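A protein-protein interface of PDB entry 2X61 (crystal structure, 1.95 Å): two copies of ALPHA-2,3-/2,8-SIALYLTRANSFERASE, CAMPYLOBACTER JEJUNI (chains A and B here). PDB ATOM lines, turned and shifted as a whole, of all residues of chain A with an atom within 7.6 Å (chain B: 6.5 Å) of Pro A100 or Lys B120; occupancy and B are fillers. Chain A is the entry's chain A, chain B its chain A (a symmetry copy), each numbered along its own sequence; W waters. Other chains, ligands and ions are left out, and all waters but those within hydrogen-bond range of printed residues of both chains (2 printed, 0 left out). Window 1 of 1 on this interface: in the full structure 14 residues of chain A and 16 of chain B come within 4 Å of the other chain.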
ATOM      1  N   TYR A  59     -17.339 -11.151 -27.193  1.00  0.00           N
ATOM      2  CA  TYR A  59     -15.949 -11.066 -27.664  1.00  0.00           C
ATOM      3  C   TYR A  59     -15.604 -12.358 -28.401  1.00  0.00           C
ATOM      4  O   TYR A  59     -15.035 -12.328 -29.484  1.00  0.00           O
ATOM      5  CB  TYR A  59     -14.991 -10.842 -26.469  1.00  0.00           C
ATOM      6  CG  TYR A  59     -13.530 -10.652 -26.824  1.00  0.00           C
ATOM      7  CD1 TYR A  59     -13.035  -9.402 -27.172  1.00  0.00           C
ATOM      8  CD2 TYR A  59     -12.638 -11.717 -26.792  1.00  0.00           C
ATOM      9  CE1 TYR A  59     -11.715  -9.223 -27.480  1.00  0.00           C
ATOM     10  CE2 TYR A  59     -11.300 -11.546 -27.098  1.00  0.00           C
ATOM     11  CZ  TYR A  59     -10.846 -10.295 -27.452  1.00  0.00           C
ATOM     12  OH  TYR A  59      -9.521 -10.094 -27.788  1.00  0.00           O
ATOM     13  N   THR A  94      -9.701  -5.889 -14.184  1.00  0.00           N
ATOM     14  CA  THR A  94      -8.800  -6.791 -14.912  1.00  0.00           C
ATOM     15  C   THR A  94      -9.018  -6.772 -16.430  1.00  0.00           C
ATOM     16  O   THR A  94      -8.388  -7.534 -17.168  1.00  0.00           O
ATOM     17  CB  THR A  94      -8.980  -8.241 -14.443  1.00  0.00           C
ATOM     18  OG1 THR A  94     -10.310  -8.682 -14.751  1.00  0.00           O
ATOM     19  CG2 THR A  94      -8.724  -8.376 -12.952  1.00  0.00           C
ATOM     20  N   PHE A  95      -9.903  -5.898 -16.892  1.00  0.00           N
ATOM     21  CA  PHE A  95     -10.318  -5.880 -18.311  1.00  0.00           C
ATOM     22  C   PHE A  95      -9.164  -5.936 -19.324  1.00  0.00           C
ATOM     23  O   PHE A  95      -9.205  -6.743 -20.259  1.00  0.00           O
ATOM     24  CB  PHE A  95     -11.155  -4.628 -18.603  1.00  0.00           C
ATOM     25  CG  PHE A  95     -11.754  -4.606 -19.991  1.00  0.00           C
ATOM     26  CD1 PHE A  95     -12.962  -5.245 -20.248  1.00  0.00           C
ATOM     27  CD2 PHE A  95     -11.097  -3.964 -21.036  1.00  0.00           C
ATOM     28  CE1 PHE A  95     -13.522  -5.238 -21.530  1.00  0.00           C
ATOM     29  CE2 PHE A  95     -11.651  -3.938 -22.324  1.00  0.00           C
ATOM     30  CZ  PHE A  95     -12.872  -4.565 -22.569  1.00  0.00           C
ATOM     31  N   TYR A  96      -8.163  -5.072 -19.172  1.00  0.00           N
ATOM     32  CA  TYR A  96      -7.119  -4.966 -20.194  1.00  0.00           C
ATOM     33  C   TYR A  96      -6.188  -6.188 -20.200  1.00  0.00           C
ATOM     34  O   TYR A  96      -5.472  -6.424 -21.176  1.00  0.00           O
ATOM     35  CB  TYR A  96      -6.340  -3.642 -20.091  1.00  0.00           C
ATOM     36  CG  TYR A  96      -7.150  -2.443 -20.576  1.00  0.00           C
ATOM     37  CD1 TYR A  96      -7.754  -1.580 -19.677  1.00  0.00           C
ATOM     38  CD2 TYR A  96      -7.354  -2.218 -21.935  1.00  0.00           C
ATOM     39  CE1 TYR A  96      -8.505  -0.495 -20.111  1.00  0.00           C
ATOM     40  CE2 TYR A  96      -8.100  -1.134 -22.383  1.00  0.00           C
ATOM     41  CZ  TYR A  96      -8.681  -0.282 -21.463  1.00  0.00           C
ATOM     42  OH  TYR A  96      -9.440   0.784 -21.890  1.00  0.00           O
ATOM     43  N   ASP A  97      -6.222  -6.987 -19.134  1.00  0.00           N
ATOM     44  CA  ASP A  97      -5.401  -8.180 -19.075  1.00  0.00           C
ATOM     45  C   ASP A  97      -6.123  -9.405 -19.644  1.00  0.00           C
ATOM     46  O   ASP A  97      -5.482 -10.367 -20.071  1.00  0.00           O
ATOM     47  CB  ASP A  97      -4.942  -8.423 -17.642  1.00  0.00           C
ATOM     48  CG  ASP A  97      -3.951  -7.365 -17.171  1.00  0.00           C
ATOM     49  OD1 ASP A  97      -3.116  -6.883 -17.973  1.00  0.00           O
ATOM     50  OD2 ASP A  97      -4.011  -7.013 -16.000  1.00  0.00           O
ATOM     51  N   TYR A  98      -7.453  -9.359 -19.677  1.00  0.00           N
ATOM     52  CA  TYR A  98      -8.235 -10.435 -20.276  1.00  0.00           C
ATOM     53  C   TYR A  98      -8.555 -10.163 -21.753  1.00  0.00           C
ATOM     54  O   TYR A  98      -8.695 -11.111 -22.541  1.00  0.00           O
ATOM     55  CB  TYR A  98      -9.518 -10.693 -19.466  1.00  0.00           C
ATOM     56  CG  TYR A  98      -9.263 -11.490 -18.206  1.00  0.00           C
ATOM     57  CD1 TYR A  98      -8.737 -10.879 -17.072  1.00  0.00           C
ATOM     58  CD2 TYR A  98      -9.504 -12.858 -18.159  1.00  0.00           C
ATOM     59  CE1 TYR A  98      -8.465 -11.599 -15.927  1.00  0.00           C
ATOM     60  CE2 TYR A  98      -9.235 -13.593 -17.017  1.00  0.00           C
ATOM     61  CZ  TYR A  98      -8.713 -12.956 -15.898  1.00  0.00           C
ATOM     62  OH  TYR A  98      -8.441 -13.663 -14.746  1.00  0.00           O
ATOM     63  N   PHE A  99      -8.657  -8.880 -22.119  1.00  0.00           N
ATOM     64  CA  PHE A  99      -9.017  -8.464 -23.480  1.00  0.00           C
ATOM     65  C   PHE A  99      -8.082  -7.341 -23.974  1.00  0.00           C
ATOM     66  O   PHE A  99      -8.490  -6.186 -24.103  1.00  0.00           O
ATOM     67  CB  PHE A  99     -10.480  -7.995 -23.538  1.00  0.00           C
ATOM     68  CG  PHE A  99     -11.454  -8.941 -22.868  1.00  0.00           C
ATOM     69  CD1 PHE A  99     -11.951  -8.657 -21.607  1.00  0.00           C
ATOM     70  CD2 PHE A  99     -11.854 -10.116 -23.497  1.00  0.00           C
ATOM     71  CE1 PHE A  99     -12.841  -9.522 -20.985  1.00  0.00           C
ATOM     72  CE2 PHE A  99     -12.727 -10.986 -22.875  1.00  0.00           C
ATOM     73  CZ  PHE A  99     -13.220 -10.695 -21.622  1.00  0.00           C
ATOM     74  N   PRO A 100      -6.813  -7.681 -24.253  1.00  0.00           N
ATOM     75  CA  PRO A 100      -5.775  -6.666 -24.459  1.00  0.00           C
ATOM     76  C   PRO A 100      -5.962  -5.767 -25.690  1.00  0.00           C
ATOM     77  O   PRO A 100      -5.380  -4.672 -25.746  1.00  0.00           O
ATOM     78  CB  PRO A 100      -4.497  -7.510 -24.573  1.00  0.00           C
ATOM     79  CG  PRO A 100      -4.835  -8.808 -23.860  1.00  0.00           C
ATOM     80  CD  PRO A 100      -6.250  -9.043 -24.231  1.00  0.00           C
ATOM     81  N   ASP A 101      -6.739  -6.220 -26.670  1.00  0.00           N
ATOM     82  CA  ASP A 101      -6.991  -5.421 -27.869  1.00  0.00           C
ATOM     83  C   ASP A 101      -8.338  -4.683 -27.829  1.00  0.00           C
ATOM     84  O   ASP A 101      -8.752  -4.077 -28.831  1.00  0.00           O
ATOM     85  CB  ASP A 101      -6.922  -6.285 -29.127  1.00  0.00           C
ATOM     86  CG  ASP A 101      -7.901  -7.450 -29.095  1.00  0.00           C
ATOM     87  OD1 ASP A 101      -8.513  -7.710 -28.025  1.00  0.00           O
ATOM     88  OD2 ASP A 101      -8.042  -8.116 -30.150  1.00  0.00           O
ATOM     89  N   ALA A 102      -9.014  -4.722 -26.679  1.00  0.00           N
ATOM     90  CA  ALA A 102     -10.278  -4.013 -26.507  1.00  0.00           C
ATOM     91  C   ALA A 102     -10.113  -2.769 -25.616  1.00  0.00           C
ATOM     92  O   ALA A 102      -9.031  -2.539 -25.062  1.00  0.00           O
ATOM     93  CB  ALA A 102     -11.342  -4.953 -25.925  1.00  0.00           C
ATOM     94  N   HIS A 103     -11.176  -1.976 -25.485  1.00  0.00           N
ATOM     95  CA  HIS A 103     -11.168  -0.797 -24.608  1.00  0.00           C
ATOM     96  C   HIS A 103     -12.409  -0.763 -23.717  1.00  0.00           C
ATOM     97  O   HIS A 103     -13.493  -1.190 -24.131  1.00  0.00           O
ATOM     98  CB  HIS A 103     -11.157   0.506 -25.424  1.00  0.00           C
ATOM     99  CG  HIS A 103      -9.874   0.771 -26.140  1.00  0.00           C
ATOM    100  ND1 HIS A 103      -9.637   0.339 -27.428  1.00  0.00           N
ATOM    101  CD2 HIS A 103      -8.754   1.427 -25.751  1.00  0.00           C
ATOM    102  CE1 HIS A 103      -8.425   0.714 -27.804  1.00  0.00           C
ATOM    103  NE2 HIS A 103      -7.866   1.374 -26.803  1.00  0.00           N
ATOM    104  N   TYR B  81       1.362 -13.711 -16.480  1.00  0.00           N
ATOM    105  CA  TYR B  81       0.409 -13.252 -17.484  1.00  0.00           C
ATOM    106  C   TYR B  81      -0.708 -12.320 -16.942  1.00  0.00           C
ATOM    107  O   TYR B  81      -1.556 -11.872 -17.724  1.00  0.00           O
ATOM    108  CB  TYR B  81      -0.271 -14.449 -18.165  1.00  0.00           C
ATOM    109  CG  TYR B  81       0.583 -15.415 -18.966  1.00  0.00           C
ATOM    110  CD1 TYR B  81       1.046 -15.081 -20.234  1.00  0.00           C
ATOM    111  CD2 TYR B  81       0.862 -16.694 -18.484  1.00  0.00           C
ATOM    112  CE1 TYR B  81       1.801 -15.976 -20.990  1.00  0.00           C
ATOM    113  CE2 TYR B  81       1.621 -17.601 -19.233  1.00  0.00           C
ATOM    114  CZ  TYR B  81       2.086 -17.222 -20.490  1.00  0.00           C
ATOM    115  OH  TYR B  81       2.803 -18.110 -21.267  1.00  0.00           O
ATOM    116  N   ASN B  82      -0.714 -12.038 -15.630  1.00  0.00           N
ATOM    117  CA  ASN B  82      -1.818 -11.311 -14.958  1.00  0.00           C
ATOM    118  C   ASN B  82      -3.153 -12.060 -15.146  1.00  0.00           C
ATOM    119  O   ASN B  82      -4.148 -11.486 -15.611  1.00  0.00           O
ATOM    120  CB  ASN B  82      -1.960  -9.850 -15.446  1.00  0.00           C
ATOM    121  CG  ASN B  82      -1.039  -8.868 -14.705  1.00  0.00           C
ATOM    122  OD1 ASN B  82      -0.070  -9.271 -14.060  1.00  0.00           O
ATOM    123  ND2 ASN B  82      -1.354  -7.577 -14.786  1.00  0.00           N
ATOM    124  N   GLN B  83      -3.149 -13.353 -14.807  1.00  0.00           N
ATOM    125  CA  GLN B  83      -4.339 -14.209 -14.894  1.00  0.00           C
ATOM    126  C   GLN B  83      -4.599 -14.894 -13.549  1.00  0.00           C
ATOM    127  O   GLN B  83      -3.755 -15.633 -13.068  1.00  0.00           O
ATOM    128  CB  GLN B  83      -4.143 -15.290 -15.971  1.00  0.00           C
ATOM    129  CG  GLN B  83      -4.066 -14.750 -17.403  1.00  0.00           C
ATOM    130  CD  GLN B  83      -5.402 -14.246 -17.881  1.00  0.00           C
ATOM    131  OE1 GLN B  83      -5.720 -13.063 -17.736  1.00  0.00           O
ATOM    132  NE2 GLN B  83      -6.213 -15.143 -18.410  1.00  0.00           N
ATOM    133  N   TYR B 106       5.640 -10.114 -17.508  1.00  0.00           N
ATOM    134  CA  TYR B 106       4.454  -9.498 -18.120  1.00  0.00           C
ATOM    135  C   TYR B 106       4.628  -8.001 -18.395  1.00  0.00           C
ATOM    136  O   TYR B 106       3.967  -7.453 -19.290  1.00  0.00           O
ATOM    137  CB  TYR B 106       3.210  -9.750 -17.258  1.00  0.00           C
ATOM    138  CG  TYR B 106       1.905  -9.417 -17.925  1.00  0.00           C
ATOM    139  CD1 TYR B 106       1.085  -8.405 -17.416  1.00  0.00           C
ATOM    140  CD2 TYR B 106       1.477 -10.102 -19.065  1.00  0.00           C
ATOM    141  CE1 TYR B 106      -0.144  -8.087 -18.025  1.00  0.00           C
ATOM    142  CE2 TYR B 106       0.252  -9.787 -19.683  1.00  0.00           C
ATOM    143  CZ  TYR B 106      -0.549  -8.785 -19.149  1.00  0.00           C
ATOM    144  OH  TYR B 106      -1.754  -8.448 -19.740  1.00  0.00           O
ATOM    145  N   PHE B 109       5.971  -8.490 -21.806  1.00  0.00           N
ATOM    146  CA  PHE B 109       5.048  -9.235 -22.647  1.00  0.00           C
ATOM    147  C   PHE B 109       3.910  -8.332 -23.103  1.00  0.00           C
ATOM    148  O   PHE B 109       3.516  -8.353 -24.277  1.00  0.00           O
ATOM    149  CB  PHE B 109       4.517 -10.437 -21.817  1.00  0.00           C
ATOM    150  CG  PHE B 109       3.709 -11.456 -22.589  1.00  0.00           C
ATOM    151  CD1 PHE B 109       2.337 -11.355 -22.670  1.00  0.00           C
ATOM    152  CD2 PHE B 109       4.317 -12.574 -23.134  1.00  0.00           C
ATOM    153  CE1 PHE B 109       1.590 -12.309 -23.328  1.00  0.00           C
ATOM    154  CE2 PHE B 109       3.586 -13.529 -23.796  1.00  0.00           C
ATOM    155  CZ  PHE B 109       2.214 -13.408 -23.881  1.00  0.00           C
ATOM    156  N   LEU B 112       3.708  -6.028 -26.244  1.00  0.00           N
ATOM    157  CA  LEU B 112       3.273  -6.570 -27.522  1.00  0.00           C
ATOM    158  C   LEU B 112       1.763  -6.792 -27.486  1.00  0.00           C
ATOM    159  O   LEU B 112       1.290  -7.890 -27.197  1.00  0.00           O
ATOM    160  CB  LEU B 112       3.987  -7.896 -27.825  1.00  0.00           C
ATOM    161  CG  LEU B 112       5.510  -7.917 -27.709  1.00  0.00           C
ATOM    162  CD1 LEU B 112       5.996  -9.247 -28.178  1.00  0.00           C
ATOM    163  CD2 LEU B 112       6.162  -6.789 -28.536  1.00  0.00           C
ATOM    164  N   LYS B 113       1.004  -5.742 -27.776  1.00  0.00           N
ATOM    165  CA  LYS B 113      -0.449  -5.787 -27.616  1.00  0.00           C
ATOM    166  C   LYS B 113      -1.113  -6.900 -28.445  1.00  0.00           C
ATOM    167  O   LYS B 113      -1.913  -7.701 -27.920  1.00  0.00           O
ATOM    168  CB  LYS B 113      -1.030  -4.418 -27.984  1.00  0.00           C
ATOM    169  CG  LYS B 113      -2.508  -4.269 -27.755  1.00  0.00           C
ATOM    170  CD  LYS B 113      -2.908  -2.774 -27.760  1.00  0.00           C
ATOM    171  CE  LYS B 113      -2.936  -2.205 -29.174  1.00  0.00           C
ATOM    172  NZ  LYS B 113      -3.435  -0.799 -29.161  1.00  0.00           N
ATOM    173  N   ASP B 114      -0.769  -6.960 -29.731  1.00  0.00           N
ATOM    174  CA  ASP B 114      -1.364  -7.947 -30.627  1.00  0.00           C
ATOM    175  C   ASP B 114      -1.065  -9.387 -30.152  1.00  0.00           C
ATOM    176  O   ASP B 114      -1.957 -10.243 -30.173  1.00  0.00           O
ATOM    177  CB  ASP B 114      -0.875  -7.739 -32.055  1.00  0.00           C
ATOM    178  CG  ASP B 114      -1.491  -6.502 -32.732  1.00  0.00           C
ATOM    179  OD1 ASP B 114      -2.361  -5.828 -32.150  1.00  0.00           O
ATOM    180  OD2 ASP B 114      -1.098  -6.216 -33.867  1.00  0.00           O
ATOM    181  N   PHE B 115       0.164  -9.648 -29.693  1.00  0.00           N
ATOM    182  CA  PHE B 115       0.482 -10.996 -29.188  1.00  0.00           C
ATOM    183  C   PHE B 115      -0.192 -11.315 -27.842  1.00  0.00           C
ATOM    184  O   PHE B 115      -0.633 -12.434 -27.632  1.00  0.00           O
ATOM    185  CB  PHE B 115       1.991 -11.239 -29.076  1.00  0.00           C
ATOM    186  CG  PHE B 115       2.337 -12.678 -28.805  1.00  0.00           C
ATOM    187  CD1 PHE B 115       2.033 -13.664 -29.745  1.00  0.00           C
ATOM    188  CD2 PHE B 115       2.934 -13.054 -27.613  1.00  0.00           C
ATOM    189  CE1 PHE B 115       2.326 -15.000 -29.500  1.00  0.00           C
ATOM    190  CE2 PHE B 115       3.237 -14.387 -27.360  1.00  0.00           C
ATOM    191  CZ  PHE B 115       2.938 -15.362 -28.302  1.00  0.00           C
ATOM    192  N   ASN B 116      -0.242 -10.343 -26.933  1.00  0.00           N
ATOM    193  CA  ASN B 116      -0.967 -10.501 -25.661  1.00  0.00           C
ATOM    194  C   ASN B 116      -2.425 -10.918 -25.954  1.00  0.00           C
ATOM    195  O   ASN B 116      -2.944 -11.866 -25.362  1.00  0.00           O
ATOM    196  CB  ASN B 116      -0.879  -9.195 -24.843  1.00  0.00           C
ATOM    197  CG  ASN B 116      -1.304  -9.354 -23.386  1.00  0.00           C
ATOM    198  OD1 ASN B 116      -1.477 -10.469 -22.871  1.00  0.00           O
ATOM    199  ND2 ASN B 116      -1.465  -8.211 -22.701  1.00  0.00           N
ATOM    200  N   ALA B 117      -3.064 -10.241 -26.898  1.00  0.00           N
ATOM    201  CA  ALA B 117      -4.442 -10.558 -27.293  1.00  0.00           C
ATOM    202  C   ALA B 117      -4.544 -11.980 -27.867  1.00  0.00           C
ATOM    203  O   ALA B 117      -5.453 -12.751 -27.520  1.00  0.00           O
ATOM    204  CB  ALA B 117      -4.934  -9.533 -28.306  1.00  0.00           C
ATOM    205  N   TYR B 118      -3.571 -12.316 -28.708  1.00  0.00           N
ATOM    206  CA  TYR B 118      -3.452 -13.643 -29.311  1.00  0.00           C
ATOM    207  C   TYR B 118      -3.354 -14.719 -28.233  1.00  0.00           C
ATOM    208  O   TYR B 118      -4.127 -15.675 -28.236  1.00  0.00           O
ATOM    209  CB  TYR B 118      -2.238 -13.663 -30.252  1.00  0.00           C
ATOM    210  CG  TYR B 118      -2.011 -14.981 -30.969  1.00  0.00           C
ATOM    211  CD1 TYR B 118      -1.316 -16.015 -30.356  1.00  0.00           C
ATOM    212  CD2 TYR B 118      -2.499 -15.193 -32.246  1.00  0.00           C
ATOM    213  CE1 TYR B 118      -1.121 -17.228 -31.000  1.00  0.00           C
ATOM    214  CE2 TYR B 118      -2.302 -16.420 -32.905  1.00  0.00           C
ATOM    215  CZ  TYR B 118      -1.617 -17.422 -32.272  1.00  0.00           C
ATOM    216  OH  TYR B 118      -1.416 -18.633 -32.911  1.00  0.00           O
ATOM    217  N   PHE B 119      -2.421 -14.550 -27.299  1.00  0.00           N
ATOM    218  CA  PHE B 119      -2.248 -15.490 -26.202  1.00  0.00           C
ATOM    219  C   PHE B 119      -3.500 -15.656 -25.336  1.00  0.00           C
ATOM    220  O   PHE B 119      -3.901 -16.786 -25.015  1.00  0.00           O
ATOM    221  CB  PHE B 119      -1.077 -15.078 -25.286  1.00  0.00           C
ATOM    222  CG  PHE B 119      -1.048 -15.857 -23.996  1.00  0.00           C
ATOM    223  CD1 PHE B 119      -0.399 -17.090 -23.930  1.00  0.00           C
ATOM    224  CD2 PHE B 119      -1.735 -15.407 -22.875  1.00  0.00           C
ATOM    225  CE1 PHE B 119      -0.432 -17.845 -22.760  1.00  0.00           C
ATOM    226  CE2 PHE B 119      -1.766 -16.155 -21.708  1.00  0.00           C
ATOM    227  CZ  PHE B 119      -1.106 -17.373 -21.647  1.00  0.00           C
ATOM    228  N   LYS B 120      -4.097 -14.536 -24.925  1.00  0.00           N
ATOM    229  CA  LYS B 120      -5.224 -14.566 -23.989  1.00  0.00           C
ATOM    230  C   LYS B 120      -6.436 -15.257 -24.598  1.00  0.00           C
ATOM    231  O   LYS B 120      -7.130 -16.036 -23.935  1.00  0.00           O
ATOM    232  CB  LYS B 120      -5.572 -13.137 -23.534  1.00  0.00           C
ATOM    233  CG  LYS B 120      -4.483 -12.500 -22.668  1.00  0.00           C
ATOM    234  CD  LYS B 120      -4.381 -13.172 -21.299  1.00  0.00           C
ATOM    235  CE  LYS B 120      -3.108 -12.773 -20.525  1.00  0.00           C
ATOM    236  NZ  LYS B 120      -2.947 -11.281 -20.350  1.00  0.00           N
ATOM    237  N   PHE B 121      -6.691 -14.995 -25.868  1.00  0.00           N
ATOM    238  CA  PHE B 121      -7.839 -15.624 -26.527  1.00  0.00           C
ATOM    239  C   PHE B 121      -7.709 -17.156 -26.544  1.00  0.00           C
ATOM    240  O   PHE B 121      -8.637 -17.877 -26.188  1.00  0.00           O
ATOM    241  CB  PHE B 121      -7.984 -15.098 -27.942  1.00  0.00           C
ATOM    242  CG  PHE B 121      -9.201 -15.616 -28.653  1.00  0.00           C
ATOM    243  CD1 PHE B 121      -9.079 -16.504 -29.707  1.00  0.00           C
ATOM    244  CD2 PHE B 121     -10.463 -15.235 -28.251  1.00  0.00           C
ATOM    245  CE1 PHE B 121     -10.203 -16.969 -30.364  1.00  0.00           C
ATOM    246  CE2 PHE B 121     -11.596 -15.720 -28.899  1.00  0.00           C
ATOM    247  CZ  PHE B 121     -11.463 -16.574 -29.946  1.00  0.00           C
ATOM    248  N   HIS B 122      -6.544 -17.645 -26.955  1.00  0.00           N
ATOM    249  CA  HIS B 122      -6.294 -19.084 -26.986  1.00  0.00           C
ATOM    250  C   HIS B 122      -6.296 -19.746 -25.598  1.00  0.00           C
ATOM    251  O   HIS B 122      -6.852 -20.834 -25.445  1.00  0.00           O
ATOM    252  CB  HIS B 122      -5.001 -19.382 -27.739  1.00  0.00           C
ATOM    253  CG  HIS B 122      -5.110 -19.141 -29.209  1.00  0.00           C
ATOM    254  ND1 HIS B 122      -4.735 -17.955 -29.801  1.00  0.00           N
ATOM    255  CD2 HIS B 122      -5.595 -19.923 -30.208  1.00  0.00           C
ATOM    256  CE1 HIS B 122      -4.968 -18.018 -31.101  1.00  0.00           C
ATOM    257  NE2 HIS B 122      -5.491 -19.201 -31.374  1.00  0.00           N
ATOM    258  N   GLU B 123      -5.700 -19.099 -24.591  1.00  0.00           N
ATOM    259  CA  GLU B 123      -5.668 -19.668 -23.223  1.00  0.00           C
ATOM    260  C   GLU B 123      -7.053 -19.733 -22.579  1.00  0.00           C
ATOM    261  O   GLU B 123      -7.483 -20.800 -22.099  1.00  0.00           O
ATOM    262  CB  GLU B 123      -4.729 -18.870 -22.306  1.00  0.00           C
ATOM    263  CG  GLU B 123      -4.955 -19.136 -20.786  1.00  0.00           C
ATOM    264  CD  GLU B 123      -4.615 -20.548 -20.389  1.00  0.00           C
ATOM    265  OE1 GLU B 123      -3.890 -21.206 -21.169  1.00  0.00           O
ATOM    266  OE2 GLU B 123      -5.089 -21.018 -19.321  1.00  0.00           O
ATOM    267  N   ILE B 124      -7.742 -18.589 -22.542  1.00  0.00           N
ATOM    268  CA  ILE B 124      -9.043 -18.483 -21.885  1.00  0.00           C
ATOM    269  C   ILE B 124     -10.124 -19.344 -22.564  1.00  0.00           C
ATOM    270  O   ILE B 124     -10.844 -20.087 -21.900  1.00  0.00           O
ATOM    271  CB  ILE B 124      -9.504 -16.995 -21.824  1.00  0.00           C
ATOM    272  CG1 ILE B 124      -8.656 -16.223 -20.807  1.00  0.00           C
ATOM    273  CG2 ILE B 124     -10.967 -16.881 -21.430  1.00  0.00           C
ATOM    274  CD1 ILE B 124      -8.530 -14.721 -21.115  1.00  0.00           C
ATOM    275  N   TYR B 125     -10.232 -19.260 -23.884  1.00  0.00           N
ATOM    276  CA  TYR B 125     -11.376 -19.870 -24.552  1.00  0.00           C
ATOM    277  C   TYR B 125     -11.121 -21.283 -25.077  1.00  0.00           C
ATOM    278  O   TYR B 125     -12.054 -22.078 -25.159  1.00  0.00           O
ATOM    279  CB  TYR B 125     -11.874 -18.975 -25.689  1.00  0.00           C
ATOM    280  CG  TYR B 125     -12.485 -17.655 -25.237  1.00  0.00           C
ATOM    281  CD1 TYR B 125     -11.728 -16.494 -25.209  1.00  0.00           C
ATOM    282  CD2 TYR B 125     -13.831 -17.572 -24.866  1.00  0.00           C
ATOM    283  CE1 TYR B 125     -12.283 -15.275 -24.801  1.00  0.00           C
ATOM    284  CE2 TYR B 125     -14.403 -16.361 -24.472  1.00  0.00           C
ATOM    285  CZ  TYR B 125     -13.623 -15.211 -24.446  1.00  0.00           C
ATOM    286  OH  TYR B 125     -14.171 -14.000 -24.068  1.00  0.00           O
ATOM    287  N   PHE B 126      -9.870 -21.601 -25.415  1.00  0.00           N
ATOM    288  CA  PHE B 126      -9.573 -22.890 -26.031  1.00  0.00           C
ATOM    289  C   PHE B 126      -8.618 -23.756 -25.234  1.00  0.00           C
ATOM    290  O   PHE B 126      -8.245 -24.829 -25.686  1.00  0.00           O
ATOM    291  CB  PHE B 126      -9.033 -22.679 -27.444  1.00  0.00           C
ATOM    292  CG  PHE B 126     -10.047 -22.103 -28.373  1.00  0.00           C
ATOM    293  CD1 PHE B 126      -9.968 -20.792 -28.779  1.00  0.00           C
ATOM    294  CD2 PHE B 126     -11.125 -22.855 -28.779  1.00  0.00           C
ATOM    295  CE1 PHE B 126     -10.927 -20.259 -29.623  1.00  0.00           C
ATOM    296  CE2 PHE B 126     -12.087 -22.320 -29.618  1.00  0.00           C
ATOM    297  CZ  PHE B 126     -11.979 -21.023 -30.038  1.00  0.00           C
HETATM  298  O   HOH W   1      -9.293 -13.087 -24.613  1.00  0.00           O
HETATM  299  O   HOH W   2      -7.641 -11.640 -26.255  1.00  0.00           O
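The side-chain carboxylate of Asp A97 sits at hydrogen-bond distance from the side-chain hydroxyl of Tyr B106 (2.7 Å).
O of Asp A97 lies within hydrogen-bond range of NZ of Lys B120 (2.7 Å).
ND2 of Asn B82 lies within hydrogen-bond range of OD2 of Asp A97, 3.0 Å away.
The side-chain amide nitrogen of Asn B116 is in hydrogen-bond range of the side-chain hydroxyl of Tyr B106, at 3.0 Å.
O of Tyr B81 sits at hydrogen-bond distance from NZ of Lys B120, 3.0 Å away.
OD1 of Asp A101 is in hydrogen-bond range of OH of Tyr A59 (2.6 Å).
OD1 of Asn B116 is in hydrogen-bond range of NZ of Lys B120, at 3.0 Å.
The side-chain hydroxyl (OH) of Tyr B106 lies within hydrogen-bond range of the side-chain amino group (NZ) of Lys B120 (3.1 Å).
Tyr A59 touches Phe B121.
Gln B83 touches Asp A97 (OE1 to O, 3.6 Å).
OE1 of Gln B83 touches CZ of Tyr A98, at 3.5 Å.
Lys B120 touches Tyr A98.
Ile B124 touches Tyr A98 (CD1 to CD2, 3.6 Å).
Phe A99 touches Tyr B125.
Pro A100 touches Lys B113 (O to CG, 3.5 Å).
Asn B116 touches Pro A100.
Ala B117 touches Pro A100 (N to CG, 3.8 Å).
Asp A101 touches Ala B117.
Printed residues of chain B within 4 Å of Tyr A98: Gln B83, Lys B120 and Ile B124.
Pro A100 touches four residues of chain B.
Printed residues of chain A within 4 Å of Asn B82: Asp A97.
Phe B109 touches none of the printed residues of chain A.
Printed residues of chain A within 4 Å of Phe B121: Tyr A59 (3.95 Å).
The nearest residue of chain B that does not touch Pro A100 is Tyr B106 (5.2 Å).
The nearest residue of chain A that does not touch Lys B120 is Phe A99 (5.4 Å).
The nearest printed residue of chain A that does not touch Lys B113 is Asp A101 (4.6 Å).
Printed residues of chain A that touch a printed residue of chain B: Tyr A59, Asp A97, Tyr A98, Phe A99, Pro A100 and Asp A101.
Among the printed residues, no Asp or Glu carboxylate lies within 4 Å of a Lys or Arg side-chain nitrogen of the other chain.
No position is printed for both chains.
Of the 15 pairs that touch across the chains among the printed residues, none has its exchanged pair printed and touching as well.
Water W2 lies within hydrogen-bond range of O of Ala B117 (2.8 Å) and OH of Tyr A59 (2.9 Å).
Water W1 lies within hydrogen-bond range of O of Tyr A98 (2.9 Å) and N of Phe B121 (3.5 Å).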
